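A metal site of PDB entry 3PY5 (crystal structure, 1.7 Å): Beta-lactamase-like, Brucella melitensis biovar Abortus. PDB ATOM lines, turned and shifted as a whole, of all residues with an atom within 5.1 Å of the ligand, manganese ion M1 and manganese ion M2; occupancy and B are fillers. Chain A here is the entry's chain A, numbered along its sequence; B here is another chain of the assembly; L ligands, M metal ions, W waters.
Merely in contact with the ligand: Ser 20, Pro 89, Tyr 129 of chain B and Tyr 139 of chain B.
Hydrophobic or aromatic side chains that line the ligand: His 90, Ala 91, His 172, His 221, His 243, Tyr 129 of chain B and Tyr 139 of chain B.
Of the 21 residues printed, 13 come within 4 Å of the ligand.
The nearest printed residue that does not touch the ligand is Pro 134 of chain B (4.1 Å).
Along chain A the residues within 4 Å of manganese ion M1 span positions 92 to 243.
The nearest printed residue that does not touch manganese ion M1 is His 88 (4.2 Å).
The guanidinium group of Arg 101 of chain B is in hydrogen-bond range of an oxygen (O7) of the ligand (2.5 Å).
OD1 of Asp 98 of chain B is in hydrogen-bond range of O7 of the ligand (2.6 Å).
A ring nitrogen (NE2) of His 221 lies within hydrogen-bond range of an oxygen (O2) of the ligand, 2.9 Å away.
The backbone NH (N) of Ala 91 is in hydrogen-bond range of a nitrogen (N5) of the ligand (3.0 Å).
Manganese ion M2 is bound by water W1 (2.0 Å), O1 of the ligand (2.1 Å), ND1 of His 90 (2.3 Å), NE2 of His 88 (2.3 Å), NE2 of His 172 (2.3 Å) and OD2 of Asp 190 (2.5 Å).
Manganese ion M2 has six donor atoms within binding distance.
A ring nitrogen (ND1) of His 172 lies within hydrogen-bond range of the backbone carbonyl oxygen of Ser 220, 2.7 Å away.
The guanidinium group of Arg 101 of chain B is in salt-bridge range of the side-chain carboxylate of Asp 98 of chain B, at 3.3 Å.
The side-chain hydroxyl of Tyr 129 of chain B lies within hydrogen-bond range of the side-chain carboxylate of Asp 98 of chain B, 2.6 Å away.
N of Tyr 139 of chain B is in hydrogen-bond range of OG of Ser 137 of chain B, 3.1 Å away.
Of the 21 residues printed, 4 come within 4 Å of manganese ion M2.
Water W1 is bound to manganese ion M1 (2.1 Å).
A ring nitrogen (NE2) of His 93 is bound to manganese ion M1, 2.2 Å away.
Manganese ion M1 is bound by NE2 of His 243.
An oxygen (O3) of the ligand is bound to manganese ion M1, at 2.2 Å.
The side-chain carboxylate (OD2) of Asp 190 binds manganese ion M1, 2.3 Å away.
OD2 of Asp 92 binds manganese ion M1, 2.3 Å away.
Manganese ion M1 has six donor atoms within binding distance.
Water W1 lies within hydrogen-bond range of OD1 of Asp 92 (2.7 Å) and O4 of the ligand (3.0 Å).
Water W7 bridges OH of Tyr 139 of chain B (2.6 Å) and OG of Ser 220 (3.1 Å).
Water W3 lies within hydrogen-bond range of O2 of the ligand and OH of Tyr 139 of chain B.
Water W8 lies within hydrogen-bond range of O2 of the ligand and N of Ser 20.
Water W5 bridges O of Pro 89 and N4 of the ligand.
Water W9 lies within hydrogen-bond range of OD2 of Asp 98 of chain B (3.0 Å), O of Ser 20 (3.0 Å) and O6 of the ligand (3.4 Å).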
ATOM      1  N   SER A  20      -6.276 -26.317  16.825  1.00  0.00           N
ATOM      2  CA  SER A  20      -6.439 -24.906  17.206  1.00  0.00           C
ATOM      3  C   SER A  20      -6.863 -23.904  16.094  1.00  0.00           C
ATOM      4  O   SER A  20      -7.554 -22.973  16.395  1.00  0.00           O
ATOM      5  CB  SER A  20      -5.239 -24.365  17.966  1.00  0.00           C
ATOM      6  OG  SER A  20      -4.090 -24.347  17.163  1.00  0.00           O
ATOM      7  N   HIS A  88      -7.381 -26.488  30.176  1.00  0.00           N
ATOM      8  CA  HIS A  88      -6.097 -25.792  30.117  1.00  0.00           C
ATOM      9  C   HIS A  88      -6.308 -24.428  29.406  1.00  0.00           C
ATOM     10  O   HIS A  88      -7.301 -24.276  28.675  1.00  0.00           O
ATOM     11  CB  HIS A  88      -4.968 -26.581  29.448  1.00  0.00           C
ATOM     12  CG  HIS A  88      -5.074 -26.700  27.945  1.00  0.00           C
ATOM     13  ND1 HIS A  88      -6.157 -27.290  27.314  1.00  0.00           N
ATOM     14  CD2 HIS A  88      -4.192 -26.393  26.962  1.00  0.00           C
ATOM     15  CE1 HIS A  88      -5.935 -27.332  26.018  1.00  0.00           C
ATOM     16  NE2 HIS A  88      -4.762 -26.785  25.767  1.00  0.00           N
ATOM     17  N   PRO A  89      -5.422 -23.460  29.660  1.00  0.00           N
ATOM     18  CA  PRO A  89      -5.650 -22.105  29.140  1.00  0.00           C
ATOM     19  C   PRO A  89      -4.959 -21.793  27.815  1.00  0.00           C
ATOM     20  O   PRO A  89      -4.007 -20.993  27.780  1.00  0.00           O
ATOM     21  CB  PRO A  89      -5.030 -21.229  30.217  1.00  0.00           C
ATOM     22  CG  PRO A  89      -3.820 -22.021  30.669  1.00  0.00           C
ATOM     23  CD  PRO A  89      -4.315 -23.485  30.650  1.00  0.00           C
ATOM     24  N   HIS A  90      -5.367 -22.474  26.775  1.00  0.00           N
ATOM     25  CA  HIS A  90      -4.939 -22.162  25.432  1.00  0.00           C
ATOM     26  C   HIS A  90      -6.141 -21.540  24.698  1.00  0.00           C
ATOM     27  O   HIS A  90      -7.302 -21.870  24.958  1.00  0.00           O
ATOM     28  CB  HIS A  90      -4.409 -23.402  24.713  1.00  0.00           C
ATOM     29  CG  HIS A  90      -2.994 -23.753  25.068  1.00  0.00           C
ATOM     30  ND1 HIS A  90      -2.412 -24.958  24.729  1.00  0.00           N
ATOM     31  CD2 HIS A  90      -2.039 -23.064  25.766  1.00  0.00           C
ATOM     32  CE1 HIS A  90      -1.158 -24.972  25.143  1.00  0.00           C
ATOM     33  NE2 HIS A  90      -0.911 -23.844  25.780  1.00  0.00           N
ATOM     34  N   ALA A  91      -5.828 -20.584  23.829  1.00  0.00           N
ATOM     35  CA  ALA A  91      -6.797 -19.796  23.046  1.00  0.00           C
ATOM     36  C   ALA A  91      -8.039 -20.586  22.563  1.00  0.00           C
ATOM     37  O   ALA A  91      -9.211 -20.175  22.740  1.00  0.00           O
ATOM     38  CB  ALA A  91      -6.053 -19.204  21.804  1.00  0.00           C
ATOM     39  N   ASP A  92      -7.764 -21.704  21.935  1.00  0.00           N
ATOM     40  CA  ASP A  92      -8.796 -22.509  21.311  1.00  0.00           C
ATOM     41  C   ASP A  92      -9.759 -23.156  22.300  1.00  0.00           C
ATOM     42  O   ASP A  92     -10.732 -23.743  21.859  1.00  0.00           O
ATOM     43  CB  ASP A  92      -8.213 -23.538  20.327  1.00  0.00           C
ATOM     44  CG  ASP A  92      -7.112 -24.417  20.921  1.00  0.00           C
ATOM     45  OD1 ASP A  92      -6.222 -23.871  21.613  1.00  0.00           O
ATOM     46  OD2 ASP A  92      -7.133 -25.618  20.593  1.00  0.00           O
ATOM     47  N   HIS A  93      -9.459 -23.059  23.607  1.00  0.00           N
ATOM     48  CA  HIS A  93     -10.250 -23.614  24.683  1.00  0.00           C
ATOM     49  C   HIS A  93     -10.879 -22.589  25.622  1.00  0.00           C
ATOM     50  O   HIS A  93     -11.753 -22.934  26.434  1.00  0.00           O
ATOM     51  CB  HIS A  93      -9.362 -24.641  25.471  1.00  0.00           C
ATOM     52  CG  HIS A  93      -8.796 -25.723  24.588  1.00  0.00           C
ATOM     53  ND1 HIS A  93      -9.341 -26.994  24.516  1.00  0.00           N
ATOM     54  CD2 HIS A  93      -7.715 -25.723  23.782  1.00  0.00           C
ATOM     55  CE1 HIS A  93      -8.615 -27.714  23.678  1.00  0.00           C
ATOM     56  NE2 HIS A  93      -7.614 -26.972  23.220  1.00  0.00           N
ATOM     57  N   ILE A  94     -10.528 -21.312  25.469  1.00  0.00           N
ATOM     58  CA  ILE A  94     -11.008 -20.321  26.401  1.00  0.00           C
ATOM     59  C   ILE A  94     -11.531 -19.003  25.795  1.00  0.00           C
ATOM     60  O   ILE A  94     -12.223 -18.273  26.485  1.00  0.00           O
ATOM     61  CB  ILE A  94      -9.921 -19.998  27.468  1.00  0.00           C
ATOM     62  CG1 ILE A  94      -8.607 -19.474  26.823  1.00  0.00           C
ATOM     63  CG2 ILE A  94      -9.718 -21.217  28.433  1.00  0.00           C
ATOM     64  CD1 ILE A  94      -7.617 -18.830  27.833  1.00  0.00           C
ATOM     65  N   HIS A  95     -11.221 -18.688  24.550  1.00  0.00           N
ATOM     66  CA  HIS A  95     -11.495 -17.361  24.028  1.00  0.00           C
ATOM     67  C   HIS A  95     -12.973 -17.070  23.675  1.00  0.00           C
ATOM     68  O   HIS A  95     -13.299 -15.962  23.264  1.00  0.00           O
ATOM     69  CB  HIS A  95     -10.554 -17.039  22.857  1.00  0.00           C
ATOM     70  CG  HIS A  95      -9.153 -16.733  23.279  1.00  0.00           C
ATOM     71  ND1 HIS A  95      -8.147 -16.490  22.370  1.00  0.00           N
ATOM     72  CD2 HIS A  95      -8.582 -16.626  24.507  1.00  0.00           C
ATOM     73  CE1 HIS A  95      -7.015 -16.255  23.019  1.00  0.00           C
ATOM     74  NE2 HIS A  95      -7.251 -16.324  24.318  1.00  0.00           N
ATOM     75  N   HIS A 172       1.031 -31.958  28.275  1.00  0.00           N
ATOM     76  CA  HIS A 172       0.665 -31.278  27.040  1.00  0.00           C
ATOM     77  C   HIS A 172       1.833 -30.412  26.597  1.00  0.00           C
ATOM     78  O   HIS A 172       1.853 -29.203  26.780  1.00  0.00           O
ATOM     79  CB  HIS A 172      -0.590 -30.442  27.303  1.00  0.00           C
ATOM     80  CG  HIS A 172      -1.090 -29.701  26.104  1.00  0.00           C
ATOM     81  ND1 HIS A 172      -0.944 -30.171  24.817  1.00  0.00           N
ATOM     82  CD2 HIS A 172      -1.755 -28.529  26.003  1.00  0.00           C
ATOM     83  CE1 HIS A 172      -1.508 -29.322  23.968  1.00  0.00           C
ATOM     84  NE2 HIS A 172      -2.015 -28.326  24.663  1.00  0.00           N
ATOM     85  N   ASP A 190      -5.627 -32.543  24.028  1.00  0.00           N
ATOM     86  CA  ASP A 190      -4.418 -31.746  24.304  1.00  0.00           C
ATOM     87  C   ASP A 190      -3.481 -32.471  25.266  1.00  0.00           C
ATOM     88  O   ASP A 190      -3.136 -31.993  26.360  1.00  0.00           O
ATOM     89  CB  ASP A 190      -4.791 -30.333  24.777  1.00  0.00           C
ATOM     90  CG  ASP A 190      -5.499 -29.528  23.704  1.00  0.00           C
ATOM     91  OD1 ASP A 190      -6.687 -29.771  23.437  1.00  0.00           O
ATOM     92  OD2 ASP A 190      -4.864 -28.656  23.125  1.00  0.00           O
ATOM     93  N   HIS A 218       4.392 -34.352  16.985  1.00  0.00           N
ATOM     94  CA  HIS A 218       4.179 -32.975  17.398  1.00  0.00           C
ATOM     95  C   HIS A 218       4.527 -32.912  18.855  1.00  0.00           C
ATOM     96  O   HIS A 218       4.252 -33.850  19.595  1.00  0.00           O
ATOM     97  CB  HIS A 218       2.728 -32.550  17.247  1.00  0.00           C
ATOM     98  CG  HIS A 218       2.510 -31.065  17.402  1.00  0.00           C
ATOM     99  ND1 HIS A 218       2.381 -30.466  18.631  1.00  0.00           N
ATOM    100  CD2 HIS A 218       2.372 -30.084  16.488  1.00  0.00           C
ATOM    101  CE1 HIS A 218       2.184 -29.162  18.457  1.00  0.00           C
ATOM    102  NE2 HIS A 218       2.165 -28.916  17.159  1.00  0.00           N
ATOM    103  N   SER A 220       3.220 -31.386  21.361  1.00  0.00           N
ATOM    104  CA  SER A 220       2.139 -31.119  22.301  1.00  0.00           C
ATOM    105  C   SER A 220       0.949 -32.067  22.193  1.00  0.00           C
ATOM    106  O   SER A 220      -0.038 -31.953  22.984  1.00  0.00           O
ATOM    107  CB  SER A 220       1.609 -29.705  22.076  1.00  0.00           C
ATOM    108  OG  SER A 220       2.643 -28.754  22.243  1.00  0.00           O
ATOM    109  N   HIS A 221       0.952 -32.930  21.180  1.00  0.00           N
ATOM    110  CA  HIS A 221      -0.169 -33.827  20.956  1.00  0.00           C
ATOM    111  C   HIS A 221       0.272 -35.146  20.458  1.00  0.00           C
ATOM    112  O   HIS A 221       1.260 -35.238  19.713  1.00  0.00           O
ATOM    113  CB  HIS A 221      -1.099 -33.285  19.893  1.00  0.00           C
ATOM    114  CG  HIS A 221      -1.600 -31.896  20.158  1.00  0.00           C
ATOM    115  ND1 HIS A 221      -2.780 -31.658  20.828  1.00  0.00           N
ATOM    116  CD2 HIS A 221      -1.107 -30.681  19.805  1.00  0.00           C
ATOM    117  CE1 HIS A 221      -2.978 -30.357  20.899  1.00  0.00           C
ATOM    118  NE2 HIS A 221      -1.969 -29.738  20.303  1.00  0.00           N
ATOM    119  N   HIS A 243      -9.527 -33.351  18.332  1.00  0.00           N
ATOM    120  CA  HIS A 243      -8.445 -32.365  18.151  1.00  0.00           C
ATOM    121  C   HIS A 243      -7.633 -32.671  16.933  1.00  0.00           C
ATOM    122  O   HIS A 243      -6.416 -32.513  16.952  1.00  0.00           O
ATOM    123  CB  HIS A 243      -7.564 -32.230  19.399  1.00  0.00           C
ATOM    124  CG  HIS A 243      -7.000 -30.878  19.610  1.00  0.00           C
ATOM    125  ND1 HIS A 243      -5.949 -30.398  18.857  1.00  0.00           N
ATOM    126  CD2 HIS A 243      -7.302 -29.894  20.494  1.00  0.00           C
ATOM    127  CE1 HIS A 243      -5.608 -29.199  19.301  1.00  0.00           C
ATOM    128  NE2 HIS A 243      -6.444 -28.854  20.260  1.00  0.00           N
ATOM    129  N   ASP B  98      -6.446 -14.609  18.118  1.00  0.00           N
ATOM    130  CA  ASP B  98      -5.481 -15.700  17.960  1.00  0.00           C
ATOM    131  C   ASP B  98      -5.512 -16.197  16.538  1.00  0.00           C
ATOM    132  O   ASP B  98      -4.507 -16.721  16.024  1.00  0.00           O
ATOM    133  CB  ASP B  98      -5.780 -16.855  18.901  1.00  0.00           C
ATOM    134  CG  ASP B  98      -4.706 -17.883  18.874  1.00  0.00           C
ATOM    135  OD1 ASP B  98      -3.691 -17.698  19.536  1.00  0.00           O
ATOM    136  OD2 ASP B  98      -4.886 -18.875  18.160  1.00  0.00           O
ATOM    137  N   ARG B 101      -2.984 -16.009  13.506  1.00  0.00           N
ATOM    138  CA  ARG B 101      -1.741 -16.783  13.417  1.00  0.00           C
ATOM    139  C   ARG B 101      -1.490 -17.377  12.039  1.00  0.00           C
ATOM    140  O   ARG B 101      -0.353 -17.343  11.567  1.00  0.00           O
ATOM    141  CB  ARG B 101      -1.785 -17.925  14.449  1.00  0.00           C
ATOM    142  CG  ARG B 101      -0.532 -18.778  14.541  1.00  0.00           C
ATOM    143  CD  ARG B 101      -0.782 -19.795  15.662  1.00  0.00           C
ATOM    144  NE  ARG B 101      -1.097 -19.042  16.875  1.00  0.00           N
ATOM    145  CZ  ARG B 101      -0.176 -18.464  17.652  1.00  0.00           C
ATOM    146  NH1 ARG B 101       1.111 -18.595  17.361  1.00  0.00           N
ATOM    147  NH2 ARG B 101      -0.537 -17.749  18.726  1.00  0.00           N
ATOM    148  N   TYR B 129       0.769 -12.927  25.003  1.00  0.00           N
ATOM    149  CA  TYR B 129       1.506 -13.931  24.246  1.00  0.00           C
ATOM    150  C   TYR B 129       1.549 -13.673  22.731  1.00  0.00           C
ATOM    151  O   TYR B 129       2.384 -14.227  22.006  1.00  0.00           O
ATOM    152  CB  TYR B 129       0.945 -15.330  24.533  1.00  0.00           C
ATOM    153  CG  TYR B 129      -0.351 -15.579  23.817  1.00  0.00           C
ATOM    154  CD1 TYR B 129      -1.549 -15.109  24.326  1.00  0.00           C
ATOM    155  CD2 TYR B 129      -0.374 -16.300  22.644  1.00  0.00           C
ATOM    156  CE1 TYR B 129      -2.722 -15.338  23.651  1.00  0.00           C
ATOM    157  CE2 TYR B 129      -1.542 -16.525  21.976  1.00  0.00           C
ATOM    158  CZ  TYR B 129      -2.724 -16.058  22.474  1.00  0.00           C
ATOM    159  OH  TYR B 129      -3.863 -16.280  21.738  1.00  0.00           O
ATOM    160  N   PRO B 134       5.851 -15.467  26.704  1.00  0.00           N
ATOM    161  CA  PRO B 134       5.951 -15.475  28.155  1.00  0.00           C
ATOM    162  C   PRO B 134       6.866 -16.535  28.710  1.00  0.00           C
ATOM    163  O   PRO B 134       7.222 -17.516  28.006  1.00  0.00           O
ATOM    164  CB  PRO B 134       4.532 -15.789  28.611  1.00  0.00           C
ATOM    165  CG  PRO B 134       3.967 -16.623  27.563  1.00  0.00           C
ATOM    166  CD  PRO B 134       4.592 -16.101  26.247  1.00  0.00           C
ATOM    167  N   SER B 137       7.167 -20.715  27.756  1.00  0.00           N
ATOM    168  CA  SER B 137       6.531 -20.963  26.435  1.00  0.00           C
ATOM    169  C   SER B 137       7.555 -20.964  25.320  1.00  0.00           C
ATOM    170  O   SER B 137       8.597 -20.324  25.399  1.00  0.00           O
ATOM    171  CB  SER B 137       5.473 -19.885  26.149  1.00  0.00           C
ATOM    172  OG  SER B 137       4.896 -20.052  24.845  1.00  0.00           O
ATOM    173  N   TYR B 139       6.110 -20.480  22.066  1.00  0.00           N
ATOM    174  CA  TYR B 139       5.355 -19.883  20.965  1.00  0.00           C
ATOM    175  C   TYR B 139       5.921 -18.493  20.636  1.00  0.00           C
ATOM    176  O   TYR B 139       5.943 -17.600  21.498  1.00  0.00           O
ATOM    177  CB  TYR B 139       3.847 -19.799  21.315  1.00  0.00           C
ATOM    178  CG  TYR B 139       3.130 -21.128  21.250  1.00  0.00           C
ATOM    179  CD1 TYR B 139       2.686 -21.646  20.048  1.00  0.00           C
ATOM    180  CD2 TYR B 139       2.875 -21.868  22.390  1.00  0.00           C
ATOM    181  CE1 TYR B 139       2.040 -22.861  19.973  1.00  0.00           C
ATOM    182  CE2 TYR B 139       2.201 -23.099  22.334  1.00  0.00           C
ATOM    183  CZ  TYR B 139       1.796 -23.584  21.122  1.00  0.00           C
ATOM    184  OH  TYR B 139       1.129 -24.776  21.009  1.00  0.00           O
HETATM  185  P1  LIG L   1      -2.825 -26.523  20.761  1.00  0.00           P
HETATM  186  O1  LIG L   1      -2.235 -26.822  22.161  1.00  0.00           O
HETATM  187  O2  LIG L   1      -1.954 -26.978  19.592  1.00  0.00           O
HETATM  188  O3  LIG L   1      -4.223 -27.051  20.477  1.00  0.00           O
HETATM  189  O4  LIG L   1      -2.924 -24.927  20.480  1.00  0.00           O
HETATM  190  C1  LIG L   1      -2.254 -23.883  21.162  1.00  0.00           C
HETATM  191  C2  LIG L   1      -3.199 -22.686  21.028  1.00  0.00           C
HETATM  192  O5  LIG L   1      -2.969 -21.798  22.115  1.00  0.00           O
HETATM  193  C3  LIG L   1      -3.016 -21.860  19.757  1.00  0.00           C
HETATM  194  O6  LIG L   1      -4.256 -21.200  19.520  1.00  0.00           O
HETATM  195  C4  LIG L   1      -1.998 -20.834  20.195  1.00  0.00           C
HETATM  196  O7  LIG L   1      -1.980 -19.681  19.351  1.00  0.00           O
HETATM  197  C5  LIG L   1      -2.506 -20.559  21.588  1.00  0.00           C
HETATM  198  N1  LIG L   1      -1.539 -20.041  22.574  1.00  0.00           N
HETATM  199  C6  LIG L   1      -0.191 -20.019  22.473  1.00  0.00           C
HETATM  200  N2  LIG L   1       0.343 -19.471  23.581  1.00  0.00           N
HETATM  201  C7  LIG L   1      -0.686 -19.128  24.391  1.00  0.00           C
HETATM  202  C8  LIG L   1      -0.795 -18.467  25.697  1.00  0.00           C
HETATM  203  N3  LIG L   1       0.278 -18.069  26.417  1.00  0.00           N
HETATM  204  N4  LIG L   1      -2.053 -18.304  26.160  1.00  0.00           N
HETATM  205  C9  LIG L   1      -3.159 -18.686  25.458  1.00  0.00           C
HETATM  206  N5  LIG L   1      -3.134 -19.272  24.253  1.00  0.00           N
HETATM  207  C10 LIG L   1      -1.921 -19.515  23.702  1.00  0.00           C
HETATM  208 MN    MN M   1      -6.033 -27.274  21.745  1.00  0.00          MN
HETATM  209 MN    MN M   2      -3.501 -26.742  23.895  1.00  0.00          MN
HETATM  210  O   HOH W   1      -4.795 -25.823  22.713  1.00  0.00           O
HETATM  211  O   HOH W   2      -2.590 -15.623  27.682  1.00  0.00           O
HETATM  212  O   HOH W   3       0.034 -25.481  18.635  1.00  0.00           O
HETATM  213  O   HOH W   4       0.473 -16.855  28.681  1.00  0.00           O
HETATM  214  O   HOH W   5      -1.449 -20.100  28.815  1.00  0.00           O
HETATM  215  O   HOH W   6       2.962 -18.449  24.478  1.00  0.00           O
HETATM  216  O   HOH W   7       0.302 -26.789  22.445  1.00  0.00           O
HETATM  217  O   HOH W   8      -3.547 -27.274  17.308  1.00  0.00           O
HETATM  218  O   HOH W   9      -7.350 -20.603  18.279  1.00  0.00           O
HETATM  219  O   HOH W  10      -3.565 -18.065  29.115  1.00  0.00           O
